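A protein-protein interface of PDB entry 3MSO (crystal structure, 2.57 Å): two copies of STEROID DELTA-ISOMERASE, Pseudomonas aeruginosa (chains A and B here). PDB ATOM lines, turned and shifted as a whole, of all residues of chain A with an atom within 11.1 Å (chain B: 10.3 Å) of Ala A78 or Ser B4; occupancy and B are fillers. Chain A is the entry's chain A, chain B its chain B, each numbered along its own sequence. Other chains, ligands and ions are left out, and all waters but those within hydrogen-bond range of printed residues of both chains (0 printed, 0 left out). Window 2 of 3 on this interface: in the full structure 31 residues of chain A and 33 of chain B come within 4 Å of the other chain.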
ATOM      1  N   LEU A   5     -37.302  24.807 -21.487  1.00  0.00           N
ATOM      2  CA  LEU A   5     -36.003  25.154 -20.901  1.00  0.00           C
ATOM      3  C   LEU A   5     -36.082  26.588 -20.321  1.00  0.00           C
ATOM      4  O   LEU A   5     -36.623  27.478 -20.994  1.00  0.00           O
ATOM      5  CB  LEU A   5     -34.934  25.045 -22.003  1.00  0.00           C
ATOM      6  CG  LEU A   5     -33.519  24.705 -21.602  1.00  0.00           C
ATOM      7  CD1 LEU A   5     -33.429  23.385 -20.840  1.00  0.00           C
ATOM      8  CD2 LEU A   5     -32.660  24.632 -22.807  1.00  0.00           C
ATOM      9  N   PRO A   6     -35.606  26.816 -19.062  1.00  0.00           N
ATOM     10  CA  PRO A   6     -35.766  28.146 -18.423  1.00  0.00           C
ATOM     11  C   PRO A   6     -34.846  29.260 -18.943  1.00  0.00           C
ATOM     12  O   PRO A   6     -34.046  29.838 -18.198  1.00  0.00           O
ATOM     13  CB  PRO A   6     -35.532  27.838 -16.945  1.00  0.00           C
ATOM     14  CG  PRO A   6     -34.541  26.720 -16.963  1.00  0.00           C
ATOM     15  CD  PRO A   6     -34.964  25.858 -18.135  1.00  0.00           C
ATOM     16  N   LEU A   7     -34.988  29.576 -20.228  1.00  0.00           N
ATOM     17  CA  LEU A   7     -34.226  30.605 -20.908  1.00  0.00           C
ATOM     18  C   LEU A   7     -34.982  31.920 -21.012  1.00  0.00           C
ATOM     19  O   LEU A   7     -36.213  31.932 -21.023  1.00  0.00           O
ATOM     20  CB  LEU A   7     -33.907  30.136 -22.321  1.00  0.00           C
ATOM     21  CG  LEU A   7     -32.886  29.024 -22.469  1.00  0.00           C
ATOM     22  CD1 LEU A   7     -32.723  28.690 -23.898  1.00  0.00           C
ATOM     23  CD2 LEU A   7     -31.534  29.404 -21.874  1.00  0.00           C
ATOM     24  N   GLU A   8     -34.238  33.023 -21.162  1.00  0.00           N
ATOM     25  CA  GLU A   8     -34.778  34.363 -21.383  1.00  0.00           C
ATOM     26  C   GLU A   8     -35.522  34.325 -22.722  1.00  0.00           C
ATOM     27  O   GLU A   8     -35.111  33.614 -23.652  1.00  0.00           O
ATOM     28  CB  GLU A   8     -33.642  35.385 -21.472  1.00  0.00           C
ATOM     29  CG  GLU A   8     -33.004  35.739 -20.146  1.00  0.00           C
ATOM     30  CD  GLU A   8     -32.077  36.943 -20.177  1.00  0.00           C
ATOM     31  OE1 GLU A   8     -31.651  37.355 -21.282  1.00  0.00           O
ATOM     32  OE2 GLU A   8     -31.743  37.452 -19.084  1.00  0.00           O
ATOM     33  N   ALA A   9     -36.609  35.078 -22.814  1.00  0.00           N
ATOM     34  CA  ALA A   9     -37.462  35.107 -23.988  1.00  0.00           C
ATOM     35  C   ALA A   9     -36.705  35.255 -25.311  1.00  0.00           C
ATOM     36  O   ALA A   9     -36.911  34.449 -26.224  1.00  0.00           O
ATOM     37  CB  ALA A   9     -38.525  36.182 -23.836  1.00  0.00           C
ATOM     38  N   ALA A  11     -33.338  34.868 -25.948  1.00  0.00           N
ATOM     39  CA  ALA A  11     -32.427  33.732 -26.062  1.00  0.00           C
ATOM     40  C   ALA A  11     -33.195  32.504 -26.565  1.00  0.00           C
ATOM     41  O   ALA A  11     -32.750  31.849 -27.512  1.00  0.00           O
ATOM     42  CB  ALA A  11     -31.819  33.451 -24.707  1.00  0.00           C
ATOM     43  N   GLN A  74     -30.336  19.039 -23.349  1.00  0.00           N
ATOM     44  CA  GLN A  74     -30.282  20.490 -23.476  1.00  0.00           C
ATOM     45  C   GLN A  74     -30.332  21.035 -22.075  1.00  0.00           C
ATOM     46  O   GLN A  74     -31.264  20.733 -21.318  1.00  0.00           O
ATOM     47  CB  GLN A  74     -31.433  21.031 -24.341  1.00  0.00           C
ATOM     48  CG  GLN A  74     -31.370  20.459 -25.754  1.00  0.00           C
ATOM     49  CD  GLN A  74     -32.300  21.115 -26.717  1.00  0.00           C
ATOM     50  OE1 GLN A  74     -32.733  22.263 -26.551  1.00  0.00           O
ATOM     51  NE2 GLN A  74     -32.596  20.395 -27.776  1.00  0.00           N
ATOM     52  N   LEU A  75     -29.282  21.787 -21.718  1.00  0.00           N
ATOM     53  CA  LEU A  75     -29.094  22.339 -20.385  1.00  0.00           C
ATOM     54  C   LEU A  75     -28.975  23.852 -20.444  1.00  0.00           C
ATOM     55  O   LEU A  75     -28.326  24.383 -21.345  1.00  0.00           O
ATOM     56  CB  LEU A  75     -27.837  21.719 -19.740  1.00  0.00           C
ATOM     57  CG  LEU A  75     -27.704  20.183 -19.802  1.00  0.00           C
ATOM     58  CD1 LEU A  75     -26.809  19.752 -20.950  1.00  0.00           C
ATOM     59  CD2 LEU A  75     -27.217  19.614 -18.488  1.00  0.00           C
ATOM     60  N   ALA A  76     -29.608  24.544 -19.495  1.00  0.00           N
ATOM     61  CA  ALA A  76     -29.617  26.005 -19.431  1.00  0.00           C
ATOM     62  C   ALA A  76     -28.962  26.488 -18.154  1.00  0.00           C
ATOM     63  O   ALA A  76     -29.128  25.872 -17.094  1.00  0.00           O
ATOM     64  CB  ALA A  76     -31.047  26.529 -19.505  1.00  0.00           C
ATOM     65  N   SER A  77     -28.235  27.621 -18.250  1.00  0.00           N
ATOM     66  CA  SER A  77     -27.608  28.255 -17.078  1.00  0.00           C
ATOM     67  C   SER A  77     -28.739  28.973 -16.285  1.00  0.00           C
ATOM     68  O   SER A  77     -29.779  29.295 -16.878  1.00  0.00           O
ATOM     69  CB  SER A  77     -26.542  29.249 -17.532  1.00  0.00           C
ATOM     70  OG  SER A  77     -27.098  30.246 -18.378  1.00  0.00           O
ATOM     71  N   ALA A  78     -28.542  29.249 -14.983  1.00  0.00           N
ATOM     72  CA  ALA A  78     -29.553  29.923 -14.153  1.00  0.00           C
ATOM     73  C   ALA A  78     -29.937  31.340 -14.625  1.00  0.00           C
ATOM     74  O   ALA A  78     -31.031  31.813 -14.309  1.00  0.00           O
ATOM     75  CB  ALA A  78     -29.101  29.967 -12.694  1.00  0.00           C
ATOM     76  N   ASP A  79     -29.059  32.013 -15.373  1.00  0.00           N
ATOM     77  CA  ASP A  79     -29.368  33.360 -15.856  1.00  0.00           C
ATOM     78  C   ASP A  79     -30.215  33.357 -17.144  1.00  0.00           C
ATOM     79  O   ASP A  79     -30.563  34.435 -17.625  1.00  0.00           O
ATOM     80  CB  ASP A  79     -28.076  34.202 -16.010  1.00  0.00           C
ATOM     81  CG  ASP A  79     -27.165  33.893 -17.187  1.00  0.00           C
ATOM     82  OD1 ASP A  79     -27.342  32.817 -17.833  1.00  0.00           O
ATOM     83  OD2 ASP A  79     -26.294  34.735 -17.490  1.00  0.00           O
ATOM     84  N   GLY A  80     -30.499  32.159 -17.691  1.00  0.00           N
ATOM     85  CA  GLY A  80     -31.257  31.979 -18.926  1.00  0.00           C
ATOM     86  C   GLY A  80     -30.626  32.589 -20.169  1.00  0.00           C
ATOM     87  O   GLY A  80     -31.332  32.877 -21.134  1.00  0.00           O
ATOM     88  N   ARG A  81     -29.286  32.785 -20.166  1.00  0.00           N
ATOM     89  CA  ARG A  81     -28.529  33.368 -21.275  1.00  0.00           C
ATOM     90  C   ARG A  81     -27.492  32.402 -21.884  1.00  0.00           C
ATOM     91  O   ARG A  81     -26.870  32.735 -22.882  1.00  0.00           O
ATOM     92  CB  ARG A  81     -27.852  34.668 -20.848  1.00  0.00           C
ATOM     93  CG  ARG A  81     -28.805  35.756 -20.448  1.00  0.00           C
ATOM     94  CD  ARG A  81     -28.073  37.070 -20.522  1.00  0.00           C
ATOM     95  NE  ARG A  81     -28.769  38.149 -19.825  1.00  0.00           N
ATOM     96  CZ  ARG A  81     -28.436  38.587 -18.616  1.00  0.00           C
ATOM     97  NH1 ARG A  81     -27.429  38.025 -17.949  1.00  0.00           N
ATOM     98  NH2 ARG A  81     -29.103  39.591 -18.063  1.00  0.00           N
ATOM     99  N   SER A  82     -27.282  31.235 -21.265  1.00  0.00           N
ATOM    100  CA  SER A  82     -26.379  30.206 -21.796  1.00  0.00           C
ATOM    101  C   SER A  82     -27.073  28.853 -21.856  1.00  0.00           C
ATOM    102  O   SER A  82     -27.853  28.492 -20.970  1.00  0.00           O
ATOM    103  CB  SER A  82     -25.077  30.112 -21.015  1.00  0.00           C
ATOM    104  OG  SER A  82     -24.129  31.068 -21.455  1.00  0.00           O
ATOM    105  N   VAL A  83     -26.778  28.118 -22.917  1.00  0.00           N
ATOM    106  CA  VAL A  83     -27.334  26.814 -23.231  1.00  0.00           C
ATOM    107  C   VAL A  83     -26.219  25.863 -23.665  1.00  0.00           C
ATOM    108  O   VAL A  83     -25.222  26.283 -24.265  1.00  0.00           O
ATOM    109  CB  VAL A  83     -28.462  26.943 -24.307  1.00  0.00           C
ATOM    110  CG1 VAL A  83     -27.917  27.065 -25.737  1.00  0.00           C
ATOM    111  CG2 VAL A  83     -29.468  25.809 -24.205  1.00  0.00           C
ATOM    112  N   VAL A  84     -26.365  24.597 -23.311  1.00  0.00           N
ATOM    113  CA  VAL A  84     -25.479  23.519 -23.757  1.00  0.00           C
ATOM    114  C   VAL A  84     -26.388  22.517 -24.482  1.00  0.00           C
ATOM    115  O   VAL A  84     -27.385  22.041 -23.914  1.00  0.00           O
ATOM    116  CB  VAL A  84     -24.599  22.868 -22.660  1.00  0.00           C
ATOM    117  CG1 VAL A  84     -24.104  21.491 -23.089  1.00  0.00           C
ATOM    118  CG2 VAL A  84     -23.427  23.757 -22.322  1.00  0.00           C
ATOM    119  N   ILE A 102     -23.619  27.689 -26.251  1.00  0.00           N
ATOM    120  CA  ILE A 102     -23.993  29.013 -26.762  1.00  0.00           C
ATOM    121  C   ILE A 102     -24.388  29.961 -25.673  1.00  0.00           C
ATOM    122  O   ILE A 102     -25.272  29.633 -24.880  1.00  0.00           O
ATOM    123  CB  ILE A 102     -25.123  28.912 -27.819  1.00  0.00           C
ATOM    124  CG1 ILE A 102     -24.886  27.742 -28.812  1.00  0.00           C
ATOM    125  CG2 ILE A 102     -25.329  30.261 -28.520  1.00  0.00           C
ATOM    126  CD1 ILE A 102     -26.137  27.218 -29.516  1.00  0.00           C
ATOM    127  N   ARG A 103     -23.739  31.151 -25.667  1.00  0.00           N
ATOM    128  CA  ARG A 103     -24.030  32.305 -24.818  1.00  0.00           C
ATOM    129  C   ARG A 103     -24.709  33.380 -25.694  1.00  0.00           C
ATOM    130  O   ARG A 103     -24.196  33.743 -26.766  1.00  0.00           O
ATOM    131  CB  ARG A 103     -22.771  32.886 -24.159  1.00  0.00           C
ATOM    132  CG  ARG A 103     -23.089  34.073 -23.208  1.00  0.00           C
ATOM    133  CD  ARG A 103     -21.850  34.831 -22.780  1.00  0.00           C
ATOM    134  NE  ARG A 103     -21.190  34.131 -21.681  1.00  0.00           N
ATOM    135  CZ  ARG A 103     -20.005  33.532 -21.778  1.00  0.00           C
ATOM    136  NH1 ARG A 103     -19.318  33.581 -22.916  1.00  0.00           N
ATOM    137  NH2 ARG A 103     -19.486  32.897 -20.729  1.00  0.00           N
ATOM    138  N   PHE A 104     -25.866  33.867 -25.226  1.00  0.00           N
ATOM    139  CA  PHE A 104     -26.687  34.911 -25.851  1.00  0.00           C
ATOM    140  C   PHE A 104     -26.573  36.192 -25.033  1.00  0.00           C
ATOM    141  O   PHE A 104     -26.405  36.108 -23.817  1.00  0.00           O
ATOM    142  CB  PHE A 104     -28.176  34.482 -25.864  1.00  0.00           C
ATOM    143  CG  PHE A 104     -28.454  33.172 -26.553  1.00  0.00           C
ATOM    144  CD1 PHE A 104     -28.688  33.123 -27.917  1.00  0.00           C
ATOM    145  CD2 PHE A 104     -28.482  31.984 -25.836  1.00  0.00           C
ATOM    146  CE1 PHE A 104     -28.931  31.904 -28.552  1.00  0.00           C
ATOM    147  CE2 PHE A 104     -28.713  30.765 -26.476  1.00  0.00           C
ATOM    148  CZ  PHE A 104     -28.931  30.733 -27.827  1.00  0.00           C
ATOM    149  N   SER B   4     -27.367  28.372  -7.263  1.00  0.00           N
ATOM    150  CA  SER B   4     -28.515  27.471  -7.296  1.00  0.00           C
ATOM    151  C   SER B   4     -29.164  27.397  -8.681  1.00  0.00           C
ATOM    152  O   SER B   4     -29.507  28.410  -9.301  1.00  0.00           O
ATOM    153  CB  SER B   4     -29.540  27.820  -6.219  1.00  0.00           C
ATOM    154  N   LEU B   5     -29.321  26.166  -9.141  1.00  0.00           N
ATOM    155  CA  LEU B   5     -29.869  25.771 -10.430  1.00  0.00           C
ATOM    156  C   LEU B   5     -31.199  25.023 -10.206  1.00  0.00           C
ATOM    157  O   LEU B   5     -31.377  24.433  -9.136  1.00  0.00           O
ATOM    158  CB  LEU B   5     -28.846  24.774 -11.041  1.00  0.00           C
ATOM    159  CG  LEU B   5     -28.071  25.109 -12.318  1.00  0.00           C
ATOM    160  CD1 LEU B   5     -27.653  26.564 -12.383  1.00  0.00           C
ATOM    161  CD2 LEU B   5     -26.847  24.233 -12.419  1.00  0.00           C
ATOM    162  N   PRO B   6     -32.079  24.913 -11.233  1.00  0.00           N
ATOM    163  CA  PRO B   6     -33.319  24.125 -11.061  1.00  0.00           C
ATOM    164  C   PRO B   6     -33.111  22.598 -11.082  1.00  0.00           C
ATOM    165  O   PRO B   6     -33.640  21.897 -11.958  1.00  0.00           O
ATOM    166  CB  PRO B   6     -34.178  24.593 -12.238  1.00  0.00           C
ATOM    167  CG  PRO B   6     -33.186  24.936 -13.309  1.00  0.00           C
ATOM    168  CD  PRO B   6     -32.011  25.533 -12.577  1.00  0.00           C
ATOM    169  N   LEU B   7     -32.336  22.085 -10.117  1.00  0.00           N
ATOM    170  CA  LEU B   7     -32.002  20.670  -9.990  1.00  0.00           C
ATOM    171  C   LEU B   7     -32.864  19.989  -8.973  1.00  0.00           C
ATOM    172  O   LEU B   7     -33.335  20.641  -8.049  1.00  0.00           O
ATOM    173  CB  LEU B   7     -30.534  20.505  -9.565  1.00  0.00           C
ATOM    174  CG  LEU B   7     -29.470  20.796 -10.589  1.00  0.00           C
ATOM    175  CD1 LEU B   7     -28.103  20.568  -9.990  1.00  0.00           C
ATOM    176  CD2 LEU B   7     -29.630  19.905 -11.831  1.00  0.00           C
ATOM    177  N   GLU B   8     -33.006  18.655  -9.088  1.00  0.00           N
ATOM    178  CA  GLU B   8     -33.699  17.824  -8.122  1.00  0.00           C
ATOM    179  C   GLU B   8     -32.927  17.930  -6.801  1.00  0.00           C
ATOM    180  O   GLU B   8     -31.700  18.042  -6.808  1.00  0.00           O
ATOM    181  CB  GLU B   8     -33.739  16.371  -8.597  1.00  0.00           C
ATOM    182  CG  GLU B   8     -34.691  16.097  -9.753  1.00  0.00           C
ATOM    183  CD  GLU B   8     -34.976  14.630 -10.029  1.00  0.00           C
ATOM    184  OE1 GLU B   8     -34.237  13.756  -9.515  1.00  0.00           O
ATOM    185  OE2 GLU B   8     -35.962  14.357 -10.751  1.00  0.00           O
ATOM    186  N   ALA B  12     -28.897  18.088  -6.475  1.00  0.00           N
ATOM    187  CA  ALA B  12     -28.350  19.332  -5.941  1.00  0.00           C
ATOM    188  C   ALA B  12     -27.439  19.073  -4.714  1.00  0.00           C
ATOM    189  O   ALA B  12     -26.368  19.678  -4.610  1.00  0.00           O
ATOM    190  CB  ALA B  12     -29.476  20.286  -5.568  1.00  0.00           C
ATOM    191  N   ALA B  13     -27.849  18.162  -3.812  1.00  0.00           N
ATOM    192  CA  ALA B  13     -27.088  17.818  -2.606  1.00  0.00           C
ATOM    193  C   ALA B  13     -25.755  17.136  -2.955  1.00  0.00           C
ATOM    194  O   ALA B  13     -24.733  17.487  -2.373  1.00  0.00           O
ATOM    195  CB  ALA B  13     -27.922  16.926  -1.706  1.00  0.00           C
ATOM    196  N   LEU B  15     -24.199  17.384  -5.946  1.00  0.00           N
ATOM    197  CA  LEU B  15     -23.430  18.424  -6.630  1.00  0.00           C
ATOM    198  C   LEU B  15     -22.731  19.320  -5.619  1.00  0.00           C
ATOM    199  O   LEU B  15     -21.535  19.571  -5.766  1.00  0.00           O
ATOM    200  CB  LEU B  15     -24.300  19.234  -7.599  1.00  0.00           C
ATOM    201  CG  LEU B  15     -23.586  20.338  -8.365  1.00  0.00           C
ATOM    202  CD1 LEU B  15     -22.524  19.761  -9.255  1.00  0.00           C
ATOM    203  CD2 LEU B  15     -24.587  21.181  -9.152  1.00  0.00           C
ATOM    204  N   ALA B  16     -23.457  19.729  -4.560  1.00  0.00           N
ATOM    205  CA  ALA B  16     -22.932  20.559  -3.468  1.00  0.00           C
ATOM    206  C   ALA B  16     -21.724  19.889  -2.800  1.00  0.00           C
ATOM    207  O   ALA B  16     -20.711  20.565  -2.543  1.00  0.00           O
ATOM    208  CB  ALA B  16     -24.021  20.826  -2.442  1.00  0.00           C
ATOM    209  N   HIS B  19     -18.779  19.713  -5.348  1.00  0.00           N
ATOM    210  CA  HIS B  19     -18.126  21.021  -5.401  1.00  0.00           C
ATOM    211  C   HIS B  19     -17.174  21.209  -4.231  1.00  0.00           C
ATOM    212  O   HIS B  19     -16.051  21.673  -4.451  1.00  0.00           O
ATOM    213  CB  HIS B  19     -19.139  22.177  -5.473  1.00  0.00           C
ATOM    214  CG  HIS B  19     -19.583  22.516  -6.857  1.00  0.00           C
ATOM    215  ND1 HIS B  19     -18.711  23.049  -7.790  1.00  0.00           N
ATOM    216  CD2 HIS B  19     -20.799  22.401  -7.420  1.00  0.00           C
ATOM    217  CE1 HIS B  19     -19.421  23.238  -8.890  1.00  0.00           C
ATOM    218  NE2 HIS B  19     -20.678  22.845  -8.725  1.00  0.00           N
ATOM    219  N   HIS B  72     -16.722  27.589 -14.080  1.00  0.00           N
ATOM    220  CA  HIS B  72     -17.315  28.806 -14.616  1.00  0.00           C
ATOM    221  C   HIS B  72     -18.833  28.664 -14.687  1.00  0.00           C
ATOM    222  O   HIS B  72     -19.450  28.622 -13.627  1.00  0.00           O
ATOM    223  CB  HIS B  72     -16.631  29.205 -15.922  1.00  0.00           C
ATOM    224  CG  HIS B  72     -15.176  29.476 -15.704  1.00  0.00           C
ATOM    225  ND1 HIS B  72     -14.752  30.558 -14.957  1.00  0.00           N
ATOM    226  CD2 HIS B  72     -14.097  28.754 -16.075  1.00  0.00           C
ATOM    227  CE1 HIS B  72     -13.436  30.478 -14.924  1.00  0.00           C
ATOM    228  NE2 HIS B  72     -12.998  29.412 -15.580  1.00  0.00           N
ATOM    229  N   ARG B  73     -19.426  28.515 -15.874  1.00  0.00           N
ATOM    230  CA  ARG B  73     -20.868  28.338 -16.021  1.00  0.00           C
ATOM    231  C   ARG B  73     -21.324  26.972 -15.560  1.00  0.00           C
ATOM    232  O   ARG B  73     -20.620  25.964 -15.725  1.00  0.00           O
ATOM    233  CB  ARG B  73     -21.317  28.536 -17.491  1.00  0.00           C
ATOM    234  CG  ARG B  73     -21.341  29.992 -17.940  1.00  0.00           C
ATOM    235  CD  ARG B  73     -21.641  30.101 -19.412  1.00  0.00           C
ATOM    236  NE  ARG B  73     -20.522  29.625 -20.232  1.00  0.00           N
ATOM    237  CZ  ARG B  73     -20.484  29.721 -21.552  1.00  0.00           C
ATOM    238  NH1 ARG B  73     -21.491  30.281 -22.213  1.00  0.00           N
ATOM    239  NH2 ARG B  73     -19.436  29.278 -22.224  1.00  0.00           N
ATOM    240  N   GLN B  74     -22.528  26.940 -14.994  1.00  0.00           N
ATOM    241  CA  GLN B  74     -23.182  25.722 -14.534  1.00  0.00           C
ATOM    242  C   GLN B  74     -24.569  25.739 -15.141  1.00  0.00           C
ATOM    243  O   GLN B  74     -25.323  26.703 -14.976  1.00  0.00           O
ATOM    244  CB  GLN B  74     -23.227  25.654 -12.999  1.00  0.00           C
ATOM    245  CG  GLN B  74     -21.825  25.645 -12.413  1.00  0.00           C
ATOM    246  CD  GLN B  74     -21.759  25.349 -10.958  1.00  0.00           C
ATOM    247  OE1 GLN B  74     -22.669  24.761 -10.380  1.00  0.00           O
ATOM    248  NE2 GLN B  74     -20.650  25.729 -10.353  1.00  0.00           N
ATOM    249  N   LEU B  75     -24.875  24.696 -15.887  1.00  0.00           N
ATOM    250  CA  LEU B  75     -26.118  24.561 -16.617  1.00  0.00           C
ATOM    251  C   LEU B  75     -26.827  23.273 -16.230  1.00  0.00           C
ATOM    252  O   LEU B  75     -26.191  22.228 -16.081  1.00  0.00           O
ATOM    253  CB  LEU B  75     -25.820  24.560 -18.139  1.00  0.00           C
ATOM    254  CG  LEU B  75     -24.899  25.684 -18.682  1.00  0.00           C
ATOM    255  CD1 LEU B  75     -23.454  25.199 -18.834  1.00  0.00           C
ATOM    256  CD2 LEU B  75     -25.431  26.248 -19.975  1.00  0.00           C
ATOM    257  N   ALA B  76     -28.146  23.344 -16.086  1.00  0.00           N
ATOM    258  CA  ALA B  76     -28.987  22.203 -15.723  1.00  0.00           C
ATOM    259  C   ALA B  76     -29.947  21.818 -16.849  1.00  0.00           C
ATOM    260  O   ALA B  76     -30.480  22.692 -17.542  1.00  0.00           O
ATOM    261  CB  ALA B  76     -29.782  22.533 -14.461  1.00  0.00           C
ATOM    262  N   SER B  77     -30.204  20.516 -17.003  1.00  0.00           N
ATOM    263  CA  SER B  77     -31.204  20.025 -17.956  1.00  0.00           C
ATOM    264  C   SER B  77     -32.619  20.283 -17.350  1.00  0.00           C
ATOM    265  O   SER B  77     -32.732  20.424 -16.118  1.00  0.00           O
ATOM    266  CB  SER B  77     -30.999  18.538 -18.209  1.00  0.00           C
ATOM    267  OG  SER B  77     -31.100  17.809 -17.000  1.00  0.00           O
ATOM    268  N   VAL B  83     -26.412  17.972 -15.164  1.00  0.00           N
ATOM    269  CA  VAL B  83     -25.681  19.210 -14.990  1.00  0.00           C
ATOM    270  C   VAL B  83     -24.451  19.237 -15.894  1.00  0.00           C
ATOM    271  O   VAL B  83     -23.857  18.189 -16.175  1.00  0.00           O
ATOM    272  CB  VAL B  83     -25.334  19.400 -13.483  1.00  0.00           C
ATOM    273  CG1 VAL B  83     -24.117  18.585 -13.041  1.00  0.00           C
ATOM    274  CG2 VAL B  83     -25.167  20.870 -13.123  1.00  0.00           C
ATOM    275  N   VAL B  84     -24.094  20.423 -16.372  1.00  0.00           N
ATOM    276  CA  VAL B  84     -22.851  20.661 -17.100  1.00  0.00           C
ATOM    277  C   VAL B  84     -22.092  21.716 -16.299  1.00  0.00           C
ATOM    278  O   VAL B  84     -22.626  22.806 -16.030  1.00  0.00           O
ATOM    279  CB  VAL B  84     -23.016  21.035 -18.600  1.00  0.00           C
ATOM    280  CG1 VAL B  84     -21.766  21.740 -19.139  1.00  0.00           C
ATOM    281  CG2 VAL B  84     -23.333  19.800 -19.433  1.00  0.00           C
ATOM    282  N   LEU B  85     -20.882  21.345 -15.857  1.00  0.00           N
ATOM    283  CA  LEU B  85     -19.989  22.234 -15.108  1.00  0.00           C
ATOM    284  C   LEU B  85     -18.833  22.595 -16.019  1.00  0.00           C
ATOM    285  O   LEU B  85     -17.981  21.742 -16.305  1.00  0.00           O
ATOM    286  CB  LEU B  85     -19.476  21.585 -13.795  1.00  0.00           C
ATOM    287  CG  LEU B  85     -20.514  20.892 -12.916  1.00  0.00           C
ATOM    288  CD1 LEU B  85     -19.850  20.111 -11.815  1.00  0.00           C
ATOM    289  CD2 LEU B  85     -21.558  21.890 -12.390  1.00  0.00           C
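Of the printed residues of chain B, Gln A74 touches Ser B77.
Of chain B, only Gln B74 and Leu B75 come within 4 Å of Ser A77.
Printed residues of chain B within 4 Å of Ala A78: Ser B4 (3.8 Å) and Leu B5 (3.7 Å).
No residue of chain B comes within 4 Å of Asp A79.
Of the printed residues of chain B, Ser A82 touches Arg B73 (2.9 Å) and Leu B75 (3.4 Å).
Of the printed residues of chain B, Val A83 touches Leu B75 (3.7 Å).
Printed residues of chain B within 4 Å of Val A84: Leu B75.
Printed residues of chain A within 4 Å of Val B83: Leu A75 (3.8 Å).
The nearest printed residue of chain A that does not touch Gln B74 is Ala A78 (4.1 Å).
Among the printed residues, pairs that only touch across the chains: Leu A75 with Ala B76 (3.2 Å), Ala A76 with Leu B75 (3.3 Å), Gln A74 with Ser B77 (3.4 Å), Ser A82 with Leu B75 (3.4 Å), Leu A75 with Ser B77 (3.5 Å), Ser A77 with Gln B74 (3.5 Å), Ser A77 with Leu B75 (3.6 Å), Leu A75 with Leu B75 (3.7 Å), Ala A78 with Leu B5 (3.7 Å), Val A83 with Leu B75 (3.7 Å), Ala A78 with Ser B4 (3.8 Å), Val A84 with Leu B75 (3.8 Å), Leu A75 with Val B84 (3.8 Å) and Leu A75 with Val B83 (3.8 Å).
The side-chain hydroxyl of Ser A77 is in hydrogen-bond range of the side-chain carboxylate of Asp A79.
N of Val B84 sits at hydrogen-bond distance from O of Leu B75 (2.8 Å).
The backbone NH of Ser A77 is in hydrogen-bond range of the backbone carbonyl oxygen of Ser A82 (2.9 Å).
The backbone NH (N) of Val A83 is in hydrogen-bond range of the backbone carbonyl oxygen (O) of Ile A102, at 2.9 Å.
The side-chain amide oxygen (OE1) of Gln B74 sits at hydrogen-bond distance from a ring nitrogen (NE2) of His B19 (3.2 Å).
The backbone carbonyl oxygen (O) of Leu A75 lies within hydrogen-bond range of the backbone NH (N) of Val A84, 2.8 Å away.
OG of Ser A82 lies within hydrogen-bond range of NH1 of Arg B73 (2.9 Å).
N of Ala A76 lies within hydrogen-bond range of O of Ala B76 (2.8 Å).
The guanidinium group (NE) of Arg B73 sits close to the guanidinium group (NH2) of Arg A103 (3.5 Å).
Leu B75 touches its own counterpart, Leu A75.
Leu A75 touches Ser B77, and with the chains exchanged Ser A77 touches Leu B75.
Leu A75 touches Val B84, and with the chains exchanged Val A84 touches Leu B75.
Ala B76 touches its own counterpart, Ala A76.
Of the 19 printed residues of chain B, 9 touch a printed residue of chain A.
Hydrophobic or aromatic side chains of chain B that line the printed part of chain A: Leu B5, Leu B75 and Val B84.
Of the 20 printed residues of chain A, 9 touch a printed residue of chain B.
Hydrophobic or aromatic side chains of chain A that line the printed part of chain B: Leu A75, Ala A78 and Val A84.
Among the printed residues, 17 pairs touch across the chains.
Among the printed residues, no Asp or Glu carboxylate lies within 4 Å of a Lys or Arg side-chain nitrogen of the other chain.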
